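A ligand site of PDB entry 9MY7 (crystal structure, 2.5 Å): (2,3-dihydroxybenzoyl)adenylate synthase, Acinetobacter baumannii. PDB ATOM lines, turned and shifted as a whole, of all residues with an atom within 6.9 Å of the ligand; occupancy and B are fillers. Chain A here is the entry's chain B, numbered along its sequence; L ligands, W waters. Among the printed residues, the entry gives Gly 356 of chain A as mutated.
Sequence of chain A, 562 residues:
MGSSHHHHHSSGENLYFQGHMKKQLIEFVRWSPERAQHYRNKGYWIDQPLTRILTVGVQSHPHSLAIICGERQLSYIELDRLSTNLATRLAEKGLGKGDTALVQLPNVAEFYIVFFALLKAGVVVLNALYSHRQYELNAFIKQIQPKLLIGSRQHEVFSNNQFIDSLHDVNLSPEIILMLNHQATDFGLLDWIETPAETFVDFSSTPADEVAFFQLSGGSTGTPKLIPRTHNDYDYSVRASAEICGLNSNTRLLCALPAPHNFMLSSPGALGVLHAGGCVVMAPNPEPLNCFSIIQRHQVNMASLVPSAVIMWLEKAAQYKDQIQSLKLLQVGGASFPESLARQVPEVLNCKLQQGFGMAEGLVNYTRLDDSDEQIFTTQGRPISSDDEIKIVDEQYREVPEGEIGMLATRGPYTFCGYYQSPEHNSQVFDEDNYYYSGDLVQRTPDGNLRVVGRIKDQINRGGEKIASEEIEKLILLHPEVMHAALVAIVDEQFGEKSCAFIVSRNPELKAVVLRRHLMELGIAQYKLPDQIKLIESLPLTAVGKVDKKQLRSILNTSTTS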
ATOM      1  N   GLY A 218      21.139   6.884  32.822  1.00  0.00           N
ATOM      2  CA  GLY A 218      19.742   7.213  33.082  1.00  0.00           C
ATOM      3  C   GLY A 218      18.839   6.409  32.171  1.00  0.00           C
ATOM      4  O   GLY A 218      19.170   6.148  31.015  1.00  0.00           O
ATOM      5  N   SER A 241      30.503  22.475  25.540  1.00  0.00           N
ATOM      6  CA  SER A 241      29.232  22.932  26.093  1.00  0.00           C
ATOM      7  C   SER A 241      29.307  24.403  26.495  1.00  0.00           C
ATOM      8  O   SER A 241      28.368  25.167  26.264  1.00  0.00           O
ATOM      9  CB  SER A 241      28.837  22.071  27.292  1.00  0.00           C
ATOM     10  OG  SER A 241      28.160  20.889  26.890  1.00  0.00           O
ATOM     11  N   HIS A 261      24.479  14.984  38.593  1.00  0.00           N
ATOM     12  CA  HIS A 261      23.912  14.629  37.307  1.00  0.00           C
ATOM     13  C   HIS A 261      24.691  15.285  36.164  1.00  0.00           C
ATOM     14  O   HIS A 261      25.092  16.445  36.262  1.00  0.00           O
ATOM     15  CB  HIS A 261      22.440  15.031  37.246  1.00  0.00           C
ATOM     16  CG  HIS A 261      21.681  14.391  36.126  1.00  0.00           C
ATOM     17  ND1 HIS A 261      20.784  13.373  36.334  1.00  0.00           N
ATOM     18  CD2 HIS A 261      21.693  14.626  34.793  1.00  0.00           C
ATOM     19  CE1 HIS A 261      20.274  12.996  35.169  1.00  0.00           C
ATOM     20  NE2 HIS A 261      20.805  13.741  34.225  1.00  0.00           N
ATOM     21  N   ASN A 262      24.900  14.516  35.090  1.00  0.00           N
ATOM     22  CA  ASN A 262      25.631  15.021  33.936  1.00  0.00           C
ATOM     23  C   ASN A 262      25.107  16.378  33.492  1.00  0.00           C
ATOM     24  O   ASN A 262      25.883  17.285  33.169  1.00  0.00           O
ATOM     25  CB  ASN A 262      25.546  14.013  32.794  1.00  0.00           C
ATOM     26  CG  ASN A 262      26.538  14.297  31.684  1.00  0.00           C
ATOM     27  OD1 ASN A 262      27.748  14.328  31.910  1.00  0.00           O
ATOM     28  ND2 ASN A 262      26.030  14.507  30.475  1.00  0.00           N
ATOM     29  N   PHE A 263      23.781  16.534  33.466  1.00  0.00           N
ATOM     30  CA  PHE A 263      23.178  17.800  33.045  1.00  0.00           C
ATOM     31  C   PHE A 263      23.663  18.955  33.911  1.00  0.00           C
ATOM     32  O   PHE A 263      24.087  19.998  33.392  1.00  0.00           O
ATOM     33  CB  PHE A 263      21.653  17.675  33.086  1.00  0.00           C
ATOM     34  CG  PHE A 263      20.934  18.840  32.470  1.00  0.00           C
ATOM     35  CD1 PHE A 263      21.351  19.373  31.265  1.00  0.00           C
ATOM     36  CD2 PHE A 263      19.794  19.359  33.069  1.00  0.00           C
ATOM     37  CE1 PHE A 263      20.663  20.432  30.686  1.00  0.00           C
ATOM     38  CE2 PHE A 263      19.106  20.412  32.503  1.00  0.00           C
ATOM     39  CZ  PHE A 263      19.545  20.946  31.307  1.00  0.00           C
ATOM     40  N   MET A 264      23.618  18.784  35.234  1.00  0.00           N
ATOM     41  CA  MET A 264      23.987  19.859  36.144  1.00  0.00           C
ATOM     42  C   MET A 264      25.500  20.028  36.292  1.00  0.00           C
ATOM     43  O   MET A 264      25.937  21.035  36.854  1.00  0.00           O
ATOM     44  CB  MET A 264      23.382  19.609  37.530  1.00  0.00           C
ATOM     45  CG  MET A 264      23.240  20.877  38.328  1.00  0.00           C
ATOM     46  SD  MET A 264      22.078  21.994  37.522  1.00  0.00           S
ATOM     47  CE  MET A 264      22.958  23.536  37.653  1.00  0.00           C
ATOM     48  N   SER A 266      28.144  19.076  33.593  1.00  0.00           N
ATOM     49  CA  SER A 266      29.042  19.181  32.445  1.00  0.00           C
ATOM     50  C   SER A 266      28.406  19.644  31.142  1.00  0.00           C
ATOM     51  O   SER A 266      29.136  19.779  30.142  1.00  0.00           O
ATOM     52  CB  SER A 266      29.717  17.815  32.196  1.00  0.00           C
ATOM     53  OG  SER A 266      28.908  16.984  31.371  1.00  0.00           O
ATOM     54  N   SER A 267      27.101  19.918  31.090  1.00  0.00           N
ATOM     55  CA  SER A 267      26.435  20.273  29.832  1.00  0.00           C
ATOM     56  C   SER A 267      25.439  21.398  30.061  1.00  0.00           C
ATOM     57  O   SER A 267      24.213  21.195  30.023  1.00  0.00           O
ATOM     58  CB  SER A 267      25.739  19.052  29.221  1.00  0.00           C
ATOM     59  OG  SER A 267      26.498  17.873  29.428  1.00  0.00           O
ATOM     60  N   PRO A 268      25.928  22.626  30.294  1.00  0.00           N
ATOM     61  CA  PRO A 268      27.329  22.994  30.539  1.00  0.00           C
ATOM     62  C   PRO A 268      27.671  22.768  32.000  1.00  0.00           C
ATOM     63  O   PRO A 268      28.797  22.423  32.349  1.00  0.00           O
ATOM     64  CB  PRO A 268      27.347  24.476  30.146  1.00  0.00           C
ATOM     65  CG  PRO A 268      25.987  24.959  30.526  1.00  0.00           C
ATOM     66  CD  PRO A 268      25.072  23.813  30.138  1.00  0.00           C
ATOM     67  N   VAL A 306      14.814  20.605  34.112  1.00  0.00           N
ATOM     68  CA  VAL A 306      14.099  19.559  33.392  1.00  0.00           C
ATOM     69  C   VAL A 306      12.654  20.015  33.199  1.00  0.00           C
ATOM     70  O   VAL A 306      12.169  20.845  33.991  1.00  0.00           O
ATOM     71  CB  VAL A 306      14.161  18.208  34.135  1.00  0.00           C
ATOM     72  CG1 VAL A 306      15.569  17.654  34.101  1.00  0.00           C
ATOM     73  CG2 VAL A 306      13.677  18.374  35.562  1.00  0.00           C
ATOM     74  N   GLN A 331      18.348  26.554  30.252  1.00  0.00           N
ATOM     75  CA  GLN A 331      18.540  25.267  29.607  1.00  0.00           C
ATOM     76  C   GLN A 331      17.414  24.330  30.025  1.00  0.00           C
ATOM     77  O   GLN A 331      17.157  24.155  31.213  1.00  0.00           O
ATOM     78  CB  GLN A 331      19.891  24.660  29.999  1.00  0.00           C
ATOM     79  CG  GLN A 331      21.018  24.965  29.049  1.00  0.00           C
ATOM     80  CD  GLN A 331      21.962  26.002  29.606  1.00  0.00           C
ATOM     81  OE1 GLN A 331      22.097  26.152  30.826  1.00  0.00           O
ATOM     82  NE2 GLN A 331      22.628  26.730  28.728  1.00  0.00           N
ATOM     83  N   VAL A 332      16.751  23.735  29.039  1.00  0.00           N
ATOM     84  CA  VAL A 332      15.710  22.757  29.290  1.00  0.00           C
ATOM     85  C   VAL A 332      16.036  21.498  28.500  1.00  0.00           C
ATOM     86  O   VAL A 332      16.217  21.559  27.280  1.00  0.00           O
ATOM     87  CB  VAL A 332      14.310  23.277  28.916  1.00  0.00           C
ATOM     88  CG1 VAL A 332      13.247  22.270  29.333  1.00  0.00           C
ATOM     89  CG2 VAL A 332      14.056  24.615  29.592  1.00  0.00           C
ATOM     90  N   GLY A 333      16.109  20.367  29.200  1.00  0.00           N
ATOM     91  CA  GLY A 333      16.310  19.078  28.554  1.00  0.00           C
ATOM     92  C   GLY A 333      15.962  17.970  29.521  1.00  0.00           C
ATOM     93  O   GLY A 333      15.669  18.202  30.694  1.00  0.00           O
ATOM     94  N   GLY A 334      15.988  16.746  29.000  1.00  0.00           N
ATOM     95  CA  GLY A 334      15.822  15.565  29.822  1.00  0.00           C
ATOM     96  C   GLY A 334      14.448  14.939  29.803  1.00  0.00           C
ATOM     97  O   GLY A 334      14.237  13.949  30.525  1.00  0.00           O
ATOM     98  N   ALA A 335      13.514  15.466  29.028  1.00  0.00           N
ATOM     99  CA  ALA A 335      12.164  14.905  28.959  1.00  0.00           C
ATOM    100  C   ALA A 335      11.429  15.563  27.797  1.00  0.00           C
ATOM    101  O   ALA A 335      11.994  16.390  27.065  1.00  0.00           O
ATOM    102  CB  ALA A 335      11.411  15.081  30.273  1.00  0.00           C
ATOM    103  N   GLY A 356      17.881  21.328  24.965  1.00  0.00           N
ATOM    104  CA  GLY A 356      18.985  20.389  24.953  1.00  0.00           C
ATOM    105  C   GLY A 356      18.498  18.963  25.066  1.00  0.00           C
ATOM    106  O   GLY A 356      17.390  18.680  25.531  1.00  0.00           O
ATOM    107  N   PHE A 357      19.362  18.048  24.631  1.00  0.00           N
ATOM    108  CA  PHE A 357      19.072  16.619  24.668  1.00  0.00           C
ATOM    109  C   PHE A 357      20.411  15.893  24.784  1.00  0.00           C
ATOM    110  O   PHE A 357      21.162  15.842  23.811  1.00  0.00           O
ATOM    111  CB  PHE A 357      18.297  16.177  23.419  1.00  0.00           C
ATOM    112  CG  PHE A 357      18.590  14.775  22.969  1.00  0.00           C
ATOM    113  CD1 PHE A 357      18.439  13.697  23.836  1.00  0.00           C
ATOM    114  CD2 PHE A 357      19.024  14.527  21.677  1.00  0.00           C
ATOM    115  CE1 PHE A 357      18.708  12.417  23.416  1.00  0.00           C
ATOM    116  CE2 PHE A 357      19.293  13.247  21.257  1.00  0.00           C
ATOM    117  CZ  PHE A 357      19.144  12.188  22.117  1.00  0.00           C
ATOM    118  N   GLY A 358      20.699  15.368  25.968  1.00  0.00           N
ATOM    119  CA  GLY A 358      21.967  14.729  26.231  1.00  0.00           C
ATOM    120  C   GLY A 358      21.785  13.393  26.932  1.00  0.00           C
ATOM    121  O   GLY A 358      20.667  12.955  27.221  1.00  0.00           O
ATOM    122  N   MET A 359      22.924  12.758  27.208  1.00  0.00           N
ATOM    123  CA  MET A 359      22.947  11.469  27.878  1.00  0.00           C
ATOM    124  C   MET A 359      24.298  11.299  28.554  1.00  0.00           C
ATOM    125  O   MET A 359      25.322  11.694  28.001  1.00  0.00           O
ATOM    126  CB  MET A 359      22.687  10.317  26.909  1.00  0.00           C
ATOM    127  CG  MET A 359      23.761  10.140  25.850  1.00  0.00           C
ATOM    128  SD  MET A 359      23.256   9.012  24.534  1.00  0.00           S
ATOM    129  CE  MET A 359      22.238  10.096  23.541  1.00  0.00           C
ATOM    130  N   ALA A 360      24.288  10.718  29.751  1.00  0.00           N
ATOM    131  CA  ALA A 360      25.528  10.506  30.488  1.00  0.00           C
ATOM    132  C   ALA A 360      26.526   9.649  29.712  1.00  0.00           C
ATOM    133  O   ALA A 360      27.723   9.713  29.991  1.00  0.00           O
ATOM    134  CB  ALA A 360      25.230   9.864  31.850  1.00  0.00           C
ATOM    135  N   GLU A 361      26.054   8.862  28.745  1.00  0.00           N
ATOM    136  CA  GLU A 361      26.943   8.033  27.961  1.00  0.00           C
ATOM    137  C   GLU A 361      27.805   8.853  27.003  1.00  0.00           C
ATOM    138  O   GLU A 361      28.847   8.360  26.556  1.00  0.00           O
ATOM    139  CB  GLU A 361      26.144   6.998  27.171  1.00  0.00           C
ATOM    140  CG  GLU A 361      25.589   5.844  28.006  1.00  0.00           C
ATOM    141  CD  GLU A 361      24.312   6.223  28.740  1.00  0.00           C
ATOM    142  OE1 GLU A 361      23.771   7.309  28.479  1.00  0.00           O
ATOM    143  OE2 GLU A 361      23.845   5.403  29.566  1.00  0.00           O
ATOM    144  N   GLY A 362      27.405  10.076  26.683  1.00  0.00           N
ATOM    145  CA  GLY A 362      28.194  10.921  25.800  1.00  0.00           C
ATOM    146  C   GLY A 362      27.429  12.010  25.089  1.00  0.00           C
ATOM    147  O   GLY A 362      27.351  13.142  25.587  1.00  0.00           O
ATOM    148  N   LEU A 363      26.855  11.685  23.933  1.00  0.00           N
ATOM    149  CA  LEU A 363      26.247  12.675  23.037  1.00  0.00           C
ATOM    150  C   LEU A 363      25.451  13.723  23.791  1.00  0.00           C
ATOM    151  O   LEU A 363      24.629  13.393  24.661  1.00  0.00           O
ATOM    152  CB  LEU A 363      25.337  11.962  22.027  1.00  0.00           C
ATOM    153  CG  LEU A 363      24.876  12.828  20.849  1.00  0.00           C
ATOM    154  CD1 LEU A 363      26.063  13.318  20.026  1.00  0.00           C
ATOM    155  CD2 LEU A 363      23.890  12.067  19.975  1.00  0.00           C
ATOM    156  N   VAL A 364      25.691  14.984  23.457  1.00  0.00           N
ATOM    157  CA  VAL A 364      24.972  16.120  24.017  1.00  0.00           C
ATOM    158  C   VAL A 364      24.538  17.020  22.877  1.00  0.00           C
ATOM    159  O   VAL A 364      25.371  17.417  22.044  1.00  0.00           O
ATOM    160  CB  VAL A 364      25.821  16.907  25.037  1.00  0.00           C
ATOM    161  CG1 VAL A 364      25.167  18.236  25.363  1.00  0.00           C
ATOM    162  CG2 VAL A 364      26.029  16.083  26.293  1.00  0.00           C
ATOM    163  N   ASN A 365      23.249  17.346  22.824  1.00  0.00           N
ATOM    164  CA  ASN A 365      22.693  18.181  21.766  1.00  0.00           C
ATOM    165  C   ASN A 365      22.166  19.483  22.347  1.00  0.00           C
ATOM    166  O   ASN A 365      21.741  19.537  23.508  1.00  0.00           O
ATOM    167  CB  ASN A 365      21.558  17.454  21.025  1.00  0.00           C
ATOM    168  CG  ASN A 365      22.042  16.216  20.295  1.00  0.00           C
ATOM    169  OD1 ASN A 365      22.409  16.282  19.127  1.00  0.00           O
ATOM    170  ND2 ASN A 365      22.055  15.088  20.990  1.00  0.00           N
ATOM    171  N   TYR A 366      22.196  20.529  21.539  1.00  0.00           N
ATOM    172  CA  TYR A 366      21.771  21.849  21.971  1.00  0.00           C
ATOM    173  C   TYR A 366      21.334  22.673  20.775  1.00  0.00           C
ATOM    174  O   TYR A 366      21.944  22.594  19.699  1.00  0.00           O
ATOM    175  CB  TYR A 366      22.895  22.578  22.713  1.00  0.00           C
ATOM    176  CG  TYR A 366      22.837  22.446  24.216  1.00  0.00           C
ATOM    177  CD1 TYR A 366      21.779  22.976  24.943  1.00  0.00           C
ATOM    178  CD2 TYR A 366      23.841  21.784  24.907  1.00  0.00           C
ATOM    179  CE1 TYR A 366      21.722  22.847  26.315  1.00  0.00           C
ATOM    180  CE2 TYR A 366      23.794  21.653  26.280  1.00  0.00           C
ATOM    181  CZ  TYR A 366      22.735  22.194  26.980  1.00  0.00           C
ATOM    182  OH  TYR A 366      22.677  22.061  28.344  1.00  0.00           O
HETATM  183  C1  LIG L   1      19.981  13.813  30.646  1.00  0.00           C
HETATM  184  O1  LIG L   1      20.421  12.672  30.422  1.00  0.00           O
HETATM  185  O2  LIG L   1      18.961  14.064  31.357  1.00  0.00           O
HETATM  186  C2  LIG L   1      20.657  14.996  30.044  1.00  0.00           C
HETATM  187  C3  LIG L   1      22.053  14.993  29.819  1.00  0.00           C
HETATM  188  C4  LIG L   1      22.683  16.106  29.250  1.00  0.00           C
HETATM  189  C5  LIG L   1      21.939  17.241  28.906  1.00  0.00           C
HETATM  190  C6  LIG L   1      20.553  17.243  29.131  1.00  0.00           C
HETATM  191  C7  LIG L   1      19.945  16.146  29.691  1.00  0.00           C
HETATM  192  O3  LIG L   1      22.783  13.934  30.134  1.00  0.00           O
HETATM  193  N1  LIG L   1      22.560  18.344  28.364  1.00  0.00           N
HETATM  194  O   HOH W   1      19.268  10.390  28.075  1.00  0.00           O
HETATM  195  O   HOH W   2      21.760  10.033  31.453  1.00  0.00           O
HETATM  196  O   HOH W   3      18.225  14.259  28.109  1.00  0.00           O
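A ring nitrogen (NE2) of His 261 lies within hydrogen-bond range of an oxygen (O2) of the ligand, 3.4 Å away. The side-chain amide nitrogen of Asn 262 lies within hydrogen-bond range of an oxygen (O3) of the ligand (3.3 Å). An oxygen (O3) of the ligand sits at hydrogen-bond distance from the backbone NH (N) of Met 359, 3.2 Å away.
The side-chain amide oxygen (OD1) of Asn 262 sits at hydrogen-bond distance from the side-chain hydroxyl (OG) of Ser 266, at 2.9 Å. OG of Ser 267 sits close to OG of Ser 266, at 3.2 Å. The backbone carbonyl oxygen of Ser 267 lies within hydrogen-bond range of the side-chain hydroxyl of Tyr 366 (2.4 Å).
The backbone carbonyl oxygen of Gly 358 sits close to an oxygen (O1) of the ligand. Residues that only touch the ligand: Phe 263 (3.1 Å), Ser 267 (3.4 Å), Gly 334 (3.8 Å), Ala 360 (3.6 Å), Val 364 (3.98 Å) and Tyr 366 (3.7 Å). Hydrophobic or aromatic side chains within 4 Å of the ligand: Phe 263 and Val 364. Within 4 Å of the ligand: His 261, Asn 262, Phe 263, Ser 267, Gly 334, Gly 358, Met 359, Ala 360, Val 364 and Tyr 366. The nearest printed residue that does not touch the ligand is Gly 333 (4.4 Å).
Water W3 lies within hydrogen-bond range of the backbone carbonyl oxygen of Gly 358 (2.9 Å), an oxygen (O2) of the ligand (3.3 Å) and the backbone NH of Gly 334 (3.5 Å). Water W2 lies within hydrogen-bond range of N of Ala 360 (3.1 Å), O1 of the ligand (3.1 Å) and N of Gly 218 (3.5 Å). Water W1 bridges the backbone carbonyl oxygen (O) of Gly 358 (3.0 Å) and an oxygen (O1) of the ligand (3.5 Å).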
